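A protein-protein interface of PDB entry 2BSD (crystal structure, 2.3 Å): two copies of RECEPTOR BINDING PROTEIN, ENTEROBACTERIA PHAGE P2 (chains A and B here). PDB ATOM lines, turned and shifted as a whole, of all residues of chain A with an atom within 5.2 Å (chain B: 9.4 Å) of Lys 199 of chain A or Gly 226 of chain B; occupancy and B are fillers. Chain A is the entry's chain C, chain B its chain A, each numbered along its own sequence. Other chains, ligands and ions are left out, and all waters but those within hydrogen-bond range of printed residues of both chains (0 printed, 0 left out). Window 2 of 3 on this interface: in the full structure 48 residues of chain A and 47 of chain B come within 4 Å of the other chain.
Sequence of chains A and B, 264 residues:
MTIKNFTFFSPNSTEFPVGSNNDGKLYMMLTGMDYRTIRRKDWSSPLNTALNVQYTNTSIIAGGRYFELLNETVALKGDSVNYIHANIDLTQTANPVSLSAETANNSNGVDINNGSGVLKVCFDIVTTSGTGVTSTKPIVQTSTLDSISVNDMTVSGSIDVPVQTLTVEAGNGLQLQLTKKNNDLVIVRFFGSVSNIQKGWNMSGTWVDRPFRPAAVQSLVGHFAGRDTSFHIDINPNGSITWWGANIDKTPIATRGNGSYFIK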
ATOM      1  N   ILE A 197      24.425 -17.486 -13.528  1.00  0.00           N
ATOM      2  CA  ILE A 197      23.934 -18.778 -13.993  1.00  0.00           C
ATOM      3  C   ILE A 197      25.088 -19.760 -14.167  1.00  0.00           C
ATOM      4  O   ILE A 197      26.215 -19.365 -14.478  1.00  0.00           O
ATOM      5  CB  ILE A 197      23.088 -18.629 -15.302  1.00  0.00           C
ATOM      6  CG1 ILE A 197      22.210 -19.865 -15.532  1.00  0.00           C
ATOM      7  CG2 ILE A 197      23.983 -18.357 -16.516  1.00  0.00           C
ATOM      8  CD1 ILE A 197      20.862 -19.571 -16.138  1.00  0.00           C
ATOM      9  N   GLN A 198      24.799 -21.036 -13.945  1.00  0.00           N
ATOM     10  CA  GLN A 198      25.770 -22.095 -14.186  1.00  0.00           C
ATOM     11  C   GLN A 198      25.297 -23.013 -15.316  1.00  0.00           C
ATOM     12  O   GLN A 198      24.099 -23.101 -15.590  1.00  0.00           O
ATOM     13  CB  GLN A 198      26.028 -22.893 -12.903  1.00  0.00           C
ATOM     14  CG  GLN A 198      26.533 -22.048 -11.726  1.00  0.00           C
ATOM     15  CD  GLN A 198      26.950 -22.880 -10.517  1.00  0.00           C
ATOM     16  OE1 GLN A 198      26.814 -24.105 -10.514  1.00  0.00           O
ATOM     17  NE2 GLN A 198      27.463 -22.210  -9.485  1.00  0.00           N
ATOM     18  N   LYS A 199      26.251 -23.671 -15.976  1.00  0.00           N
ATOM     19  CA  LYS A 199      25.950 -24.703 -16.973  1.00  0.00           C
ATOM     20  C   LYS A 199      24.963 -25.732 -16.423  1.00  0.00           C
ATOM     21  O   LYS A 199      25.130 -26.229 -15.309  1.00  0.00           O
ATOM     22  CB  LYS A 199      27.239 -25.399 -17.451  1.00  0.00           C
ATOM     23  CG  LYS A 199      28.127 -25.973 -16.334  1.00  0.00           C
ATOM     24  CD  LYS A 199      29.352 -26.702 -16.876  1.00  0.00           C
ATOM     25  CE  LYS A 199      30.554 -25.767 -16.982  1.00  0.00           C
ATOM     26  NZ  LYS A 199      31.402 -25.787 -15.760  1.00  0.00           N
ATOM     27  N   GLY A 200      23.924 -26.025 -17.204  1.00  0.00           N
ATOM     28  CA  GLY A 200      22.912 -26.998 -16.827  1.00  0.00           C
ATOM     29  C   GLY A 200      21.784 -26.493 -15.939  1.00  0.00           C
ATOM     30  O   GLY A 200      20.868 -27.243 -15.624  1.00  0.00           O
ATOM     31  N   TRP A 201      21.859 -25.230 -15.523  1.00  0.00           N
ATOM     32  CA  TRP A 201      20.768 -24.596 -14.797  1.00  0.00           C
ATOM     33  C   TRP A 201      19.679 -24.143 -15.766  1.00  0.00           C
ATOM     34  O   TRP A 201      19.969 -23.558 -16.819  1.00  0.00           O
ATOM     35  CB  TRP A 201      21.266 -23.382 -14.002  1.00  0.00           C
ATOM     36  CG  TRP A 201      22.004 -23.690 -12.730  1.00  0.00           C
ATOM     37  CD1 TRP A 201      22.429 -24.910 -12.291  1.00  0.00           C
ATOM     38  CD2 TRP A 201      22.408 -22.748 -11.735  1.00  0.00           C
ATOM     39  NE1 TRP A 201      23.070 -24.788 -11.083  1.00  0.00           N
ATOM     40  CE2 TRP A 201      23.071 -23.469 -10.716  1.00  0.00           C
ATOM     41  CE3 TRP A 201      22.270 -21.360 -11.592  1.00  0.00           C
ATOM     42  CZ2 TRP A 201      23.597 -22.852  -9.576  1.00  0.00           C
ATOM     43  CZ3 TRP A 201      22.792 -20.747 -10.460  1.00  0.00           C
ATOM     44  CH2 TRP A 201      23.445 -21.494  -9.464  1.00  0.00           C
ATOM     45  N   TRP A 243      20.564 -23.382 -19.679  1.00  0.00           N
ATOM     46  CA  TRP A 243      21.813 -22.725 -20.032  1.00  0.00           C
ATOM     47  C   TRP A 243      22.948 -23.737 -20.208  1.00  0.00           C
ATOM     48  O   TRP A 243      23.205 -24.549 -19.316  1.00  0.00           O
ATOM     49  CB  TRP A 243      22.196 -21.722 -18.952  1.00  0.00           C
ATOM     50  CG  TRP A 243      23.471 -20.993 -19.240  1.00  0.00           C
ATOM     51  CD1 TRP A 243      24.705 -21.236 -18.695  1.00  0.00           C
ATOM     52  CD2 TRP A 243      23.640 -19.891 -20.136  1.00  0.00           C
ATOM     53  NE1 TRP A 243      25.626 -20.348 -19.198  1.00  0.00           N
ATOM     54  CE2 TRP A 243      25.001 -19.513 -20.088  1.00  0.00           C
ATOM     55  CE3 TRP A 243      22.777 -19.178 -20.983  1.00  0.00           C
ATOM     56  CZ2 TRP A 243      25.520 -18.459 -20.857  1.00  0.00           C
ATOM     57  CZ3 TRP A 243      23.292 -18.128 -21.739  1.00  0.00           C
ATOM     58  CH2 TRP A 243      24.650 -17.780 -21.667  1.00  0.00           C
ATOM     59  N   TRP A 244      23.628 -23.674 -21.349  1.00  0.00           N
ATOM     60  CA  TRP A 244      24.778 -24.540 -21.606  1.00  0.00           C
ATOM     61  C   TRP A 244      25.994 -23.776 -22.130  1.00  0.00           C
ATOM     62  O   TRP A 244      26.834 -24.341 -22.839  1.00  0.00           O
ATOM     63  CB  TRP A 244      24.409 -25.690 -22.552  1.00  0.00           C
ATOM     64  CG  TRP A 244      23.578 -26.758 -21.899  1.00  0.00           C
ATOM     65  CD1 TRP A 244      22.286 -27.083 -22.194  1.00  0.00           C
ATOM     66  CD2 TRP A 244      23.976 -27.633 -20.832  1.00  0.00           C
ATOM     67  NE1 TRP A 244      21.858 -28.109 -21.385  1.00  0.00           N
ATOM     68  CE2 TRP A 244      22.872 -28.465 -20.536  1.00  0.00           C
ATOM     69  CE3 TRP A 244      25.160 -27.803 -20.093  1.00  0.00           C
ATOM     70  CZ2 TRP A 244      22.914 -29.456 -19.542  1.00  0.00           C
ATOM     71  CZ3 TRP A 244      25.199 -28.787 -19.096  1.00  0.00           C
ATOM     72  CH2 TRP A 244      24.083 -29.601 -18.839  1.00  0.00           C
ATOM     73  N   GLY A 245      26.075 -22.491 -21.794  1.00  0.00           N
ATOM     74  CA  GLY A 245      27.322 -21.759 -21.923  1.00  0.00           C
ATOM     75  C   GLY A 245      28.161 -22.055 -20.690  1.00  0.00           C
ATOM     76  O   GLY A 245      27.801 -22.926 -19.888  1.00  0.00           O
ATOM     77  N   ALA A 246      29.271 -21.345 -20.516  1.00  0.00           N
ATOM     78  CA  ALA A 246      30.054 -21.479 -19.287  1.00  0.00           C
ATOM     79  C   ALA A 246      29.319 -20.816 -18.122  1.00  0.00           C
ATOM     80  O   ALA A 246      28.288 -20.169 -18.326  1.00  0.00           O
ATOM     81  CB  ALA A 246      31.453 -20.887 -19.464  1.00  0.00           C
ATOM     82  N   ASN A 247      29.828 -21.007 -16.904  1.00  0.00           N
ATOM     83  CA  ASN A 247      29.324 -20.292 -15.731  1.00  0.00           C
ATOM     84  C   ASN A 247      29.554 -18.795 -15.861  1.00  0.00           C
ATOM     85  O   ASN A 247      30.654 -18.359 -16.202  1.00  0.00           O
ATOM     86  CB  ASN A 247      29.993 -20.790 -14.444  1.00  0.00           C
ATOM     87  CG  ASN A 247      29.697 -22.248 -14.149  1.00  0.00           C
ATOM     88  OD1 ASN A 247      28.854 -22.878 -14.791  1.00  0.00           O
ATOM     89  ND2 ASN A 247      30.400 -22.795 -13.168  1.00  0.00           N
ATOM     90  N   HIS B 223      28.547 -25.505 -30.993  1.00  0.00           N
ATOM     91  CA  HIS B 223      28.966 -25.003 -29.697  1.00  0.00           C
ATOM     92  C   HIS B 223      29.364 -26.150 -28.778  1.00  0.00           C
ATOM     93  O   HIS B 223      28.768 -27.234 -28.831  1.00  0.00           O
ATOM     94  CB  HIS B 223      27.852 -24.168 -29.051  1.00  0.00           C
ATOM     95  CG  HIS B 223      28.261 -23.540 -27.760  1.00  0.00           C
ATOM     96  ND1 HIS B 223      27.893 -24.052 -26.536  1.00  0.00           N
ATOM     97  CD2 HIS B 223      29.049 -22.471 -27.500  1.00  0.00           C
ATOM     98  CE1 HIS B 223      28.418 -23.314 -25.574  1.00  0.00           C
ATOM     99  NE2 HIS B 223      29.132 -22.351 -26.133  1.00  0.00           N
ATOM    100  N   PHE B 224      30.371 -25.904 -27.944  1.00  0.00           N
ATOM    101  CA  PHE B 224      30.810 -26.869 -26.943  1.00  0.00           C
ATOM    102  C   PHE B 224      30.058 -26.621 -25.643  1.00  0.00           C
ATOM    103  O   PHE B 224      30.276 -25.602 -24.981  1.00  0.00           O
ATOM    104  CB  PHE B 224      32.321 -26.758 -26.702  1.00  0.00           C
ATOM    105  CG  PHE B 224      33.166 -27.178 -27.879  1.00  0.00           C
ATOM    106  CD1 PHE B 224      33.173 -28.500 -28.321  1.00  0.00           C
ATOM    107  CD2 PHE B 224      33.968 -26.250 -28.537  1.00  0.00           C
ATOM    108  CE1 PHE B 224      33.968 -28.889 -29.398  1.00  0.00           C
ATOM    109  CE2 PHE B 224      34.773 -26.627 -29.623  1.00  0.00           C
ATOM    110  CZ  PHE B 224      34.769 -27.947 -30.056  1.00  0.00           C
ATOM    111  N   ALA B 225      29.189 -27.567 -25.283  1.00  0.00           N
ATOM    112  CA  ALA B 225      28.347 -27.504 -24.087  1.00  0.00           C
ATOM    113  C   ALA B 225      29.131 -27.251 -22.799  1.00  0.00           C
ATOM    114  O   ALA B 225      30.136 -27.902 -22.534  1.00  0.00           O
ATOM    115  CB  ALA B 225      27.538 -28.790 -23.959  1.00  0.00           C
ATOM    116  N   GLY B 226      28.653 -26.298 -22.004  1.00  0.00           N
ATOM    117  CA  GLY B 226      29.296 -25.940 -20.756  1.00  0.00           C
ATOM    118  C   GLY B 226      30.552 -25.099 -20.938  1.00  0.00           C
ATOM    119  O   GLY B 226      31.268 -24.840 -19.976  1.00  0.00           O
ATOM    120  N   ARG B 227      30.815 -24.663 -22.167  1.00  0.00           N
ATOM    121  CA  ARG B 227      32.008 -23.874 -22.453  1.00  0.00           C
ATOM    122  C   ARG B 227      31.647 -22.590 -23.205  1.00  0.00           C
ATOM    123  O   ARG B 227      30.493 -22.392 -23.579  1.00  0.00           O
ATOM    124  CB  ARG B 227      33.022 -24.714 -23.235  1.00  0.00           C
ATOM    125  CG  ARG B 227      33.784 -25.711 -22.375  1.00  0.00           C
ATOM    126  CD  ARG B 227      34.532 -26.769 -23.167  1.00  0.00           C
ATOM    127  NE  ARG B 227      34.959 -27.886 -22.322  1.00  0.00           N
ATOM    128  CZ  ARG B 227      36.198 -28.363 -22.267  1.00  0.00           C
ATOM    129  NH1 ARG B 227      37.165 -27.821 -23.000  1.00  0.00           N
ATOM    130  NH2 ARG B 227      36.477 -29.387 -21.472  1.00  0.00           N
ATOM    131  N   ASP B 228      32.624 -21.710 -23.406  1.00  0.00           N
ATOM    132  CA  ASP B 228      32.378 -20.494 -24.178  1.00  0.00           C
ATOM    133  C   ASP B 228      33.009 -20.553 -25.580  1.00  0.00           C
ATOM    134  O   ASP B 228      33.164 -19.534 -26.260  1.00  0.00           O
ATOM    135  CB  ASP B 228      32.778 -19.236 -23.389  1.00  0.00           C
ATOM    136  CG  ASP B 228      34.265 -19.153 -23.113  1.00  0.00           C
ATOM    137  OD1 ASP B 228      35.059 -19.818 -23.816  1.00  0.00           O
ATOM    138  OD2 ASP B 228      34.738 -18.434 -22.206  1.00  0.00           O
ATOM    139  N   THR B 229      33.348 -21.770 -25.997  1.00  0.00           N
ATOM    140  CA  THR B 229      34.066 -22.010 -27.239  1.00  0.00           C
ATOM    141  C   THR B 229      33.163 -22.595 -28.322  1.00  0.00           C
ATOM    142  O   THR B 229      32.096 -23.145 -28.044  1.00  0.00           O
ATOM    143  CB  THR B 229      35.269 -22.943 -27.007  1.00  0.00           C
ATOM    144  OG1 THR B 229      34.828 -24.137 -26.354  1.00  0.00           O
ATOM    145  CG2 THR B 229      36.274 -22.322 -26.016  1.00  0.00           C
ATOM    146  N   ILE B 253      34.743 -33.651 -26.053  1.00  0.00           N
ATOM    147  CA  ILE B 253      33.964 -32.483 -25.643  1.00  0.00           C
ATOM    148  C   ILE B 253      32.601 -32.533 -26.327  1.00  0.00           C
ATOM    149  O   ILE B 253      32.530 -32.670 -27.549  1.00  0.00           O
ATOM    150  CB  ILE B 253      34.693 -31.156 -25.986  1.00  0.00           C
ATOM    151  CG1 ILE B 253      36.149 -31.188 -25.506  1.00  0.00           C
ATOM    152  CG2 ILE B 253      33.959 -29.967 -25.360  1.00  0.00           C
ATOM    153  CD1 ILE B 253      37.110 -30.437 -26.417  1.00  0.00           C
ATOM    154  N   ALA B 254      31.536 -32.426 -25.529  1.00  0.00           N
ATOM    155  CA  ALA B 254      30.159 -32.462 -26.023  1.00  0.00           C
ATOM    156  C   ALA B 254      29.862 -31.343 -27.035  1.00  0.00           C
ATOM    157  O   ALA B 254      30.118 -30.159 -26.771  1.00  0.00           O
ATOM    158  CB  ALA B 254      29.167 -32.419 -24.854  1.00  0.00           C
ATOM    159  N   THR B 255      29.330 -31.738 -28.192  1.00  0.00           N
ATOM    160  CA  THR B 255      29.053 -30.827 -29.306  1.00  0.00           C
ATOM    161  C   THR B 255      27.554 -30.665 -29.527  1.00  0.00           C
ATOM    162  O   THR B 255      26.818 -31.657 -29.606  1.00  0.00           O
ATOM    163  CB  THR B 255      29.699 -31.368 -30.606  1.00  0.00           C
ATOM    164  OG1 THR B 255      29.393 -32.763 -30.749  1.00  0.00           O
ATOM    165  CG2 THR B 255      31.225 -31.330 -30.520  1.00  0.00           C
ATOM    166  N   ARG B 256      27.099 -29.418 -29.640  1.00  0.00           N
ATOM    167  CA  ARG B 256      25.671 -29.129 -29.759  1.00  0.00           C
ATOM    168  C   ARG B 256      25.406 -27.952 -30.693  1.00  0.00           C
ATOM    169  O   ARG B 256      26.318 -27.187 -31.019  1.00  0.00           O
ATOM    170  CB  ARG B 256      25.048 -28.840 -28.380  1.00  0.00           C
ATOM    171  CG  ARG B 256      25.121 -29.981 -27.352  1.00  0.00           C
ATOM    172  CD  ARG B 256      24.164 -31.157 -27.604  1.00  0.00           C
ATOM    173  NE  ARG B 256      24.244 -32.154 -26.533  1.00  0.00           N
ATOM    174  CZ  ARG B 256      25.166 -33.115 -26.459  1.00  0.00           C
ATOM    175  NH1 ARG B 256      26.103 -33.225 -27.399  1.00  0.00           N
ATOM    176  NH2 ARG B 256      25.163 -33.961 -25.436  1.00  0.00           N
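The backbone carbonyl oxygen of Arg 227 of chain B is in hydrogen-bond range of a ring nitrogen (NE2) of His 223 of chain B, at 2.9 Å.
N of His 223 of chain B lies within hydrogen-bond range of O of Arg 256 of chain B, at 2.8 Å.
The backbone NH of Ala 225 of chain B is in hydrogen-bond range of the backbone carbonyl oxygen of Ala 254 of chain B, 3.1 Å away.
OD1 of Asn 247 of chain A sits at hydrogen-bond distance from N of Lys 199 of chain A (3.0 Å).
O of Gly 245 of chain A lies close to NE1 of Trp 243 of chain A (3.4 Å).
NE1 of Trp 243 of chain A lies within hydrogen-bond range of O of Ala 246 of chain A, at 2.8 Å.
The backbone NH of Gly 226 of chain B is in hydrogen-bond range of the backbone carbonyl oxygen of Trp 244 of chain A (2.8 Å).
The backbone NH (N) of Ala 246 of chain A sits at hydrogen-bond distance from the backbone carbonyl oxygen (O) of Arg 227 of chain B (3.5 Å).
O of Gly 226 of chain B touches CE of Lys 199 of chain A, at 3.2 Å.
His 223 of chain B touches Trp 244 of chain A (CE1 to O, 3.3 Å).
C of Ala 225 of chain B touches O of Trp 244 of chain A, at 3.7 Å.
Gly 226 of chain B touches Gly 245 of chain A (CA to O, 3.5 Å).
Gly 245 of chain A touches Arg 227 of chain B (CA to O, 3.6 Å).
O of Gly 226 of chain B touches CA of Ala 246 of chain A, 3.6 Å away.
Hydrophobic or aromatic side chains of chain B within 4 Å of the printed part of chain A: His 223.
Of the 10 printed residues of chain A, 4 touch a printed residue of chain B.
Hydrophobic or aromatic side chains of chain A that line the printed part of chain B: Ala 246.
No position is printed for both chains.
Of the 8 pairs that touch across the chains among the printed residues, none has its exchanged pair printed and touching as well.
Of chain B, only Gly 226 (3.2 Å) comes within 4 Å of Lys 199 of chain A.
Gly 226 of chain B touches four residues of chain A.
Gly 245 of chain A touches just these residues of chain B: Gly 226 and Arg 227.
Of chain B, only Gly 226 (3.6 Å) and Arg 227 (3.5 Å) come within 4 Å of Ala 246 of chain A.
Printed residues of chain A within 4 Å of Arg 227 of chain B: Gly 245 (3.6 Å) and Ala 246 (3.5 Å).
Of the printed residues of chain A, Ala 225 of chain B touches Trp 244.
Gln 198 of chain A touches none of the printed residues of chain B.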
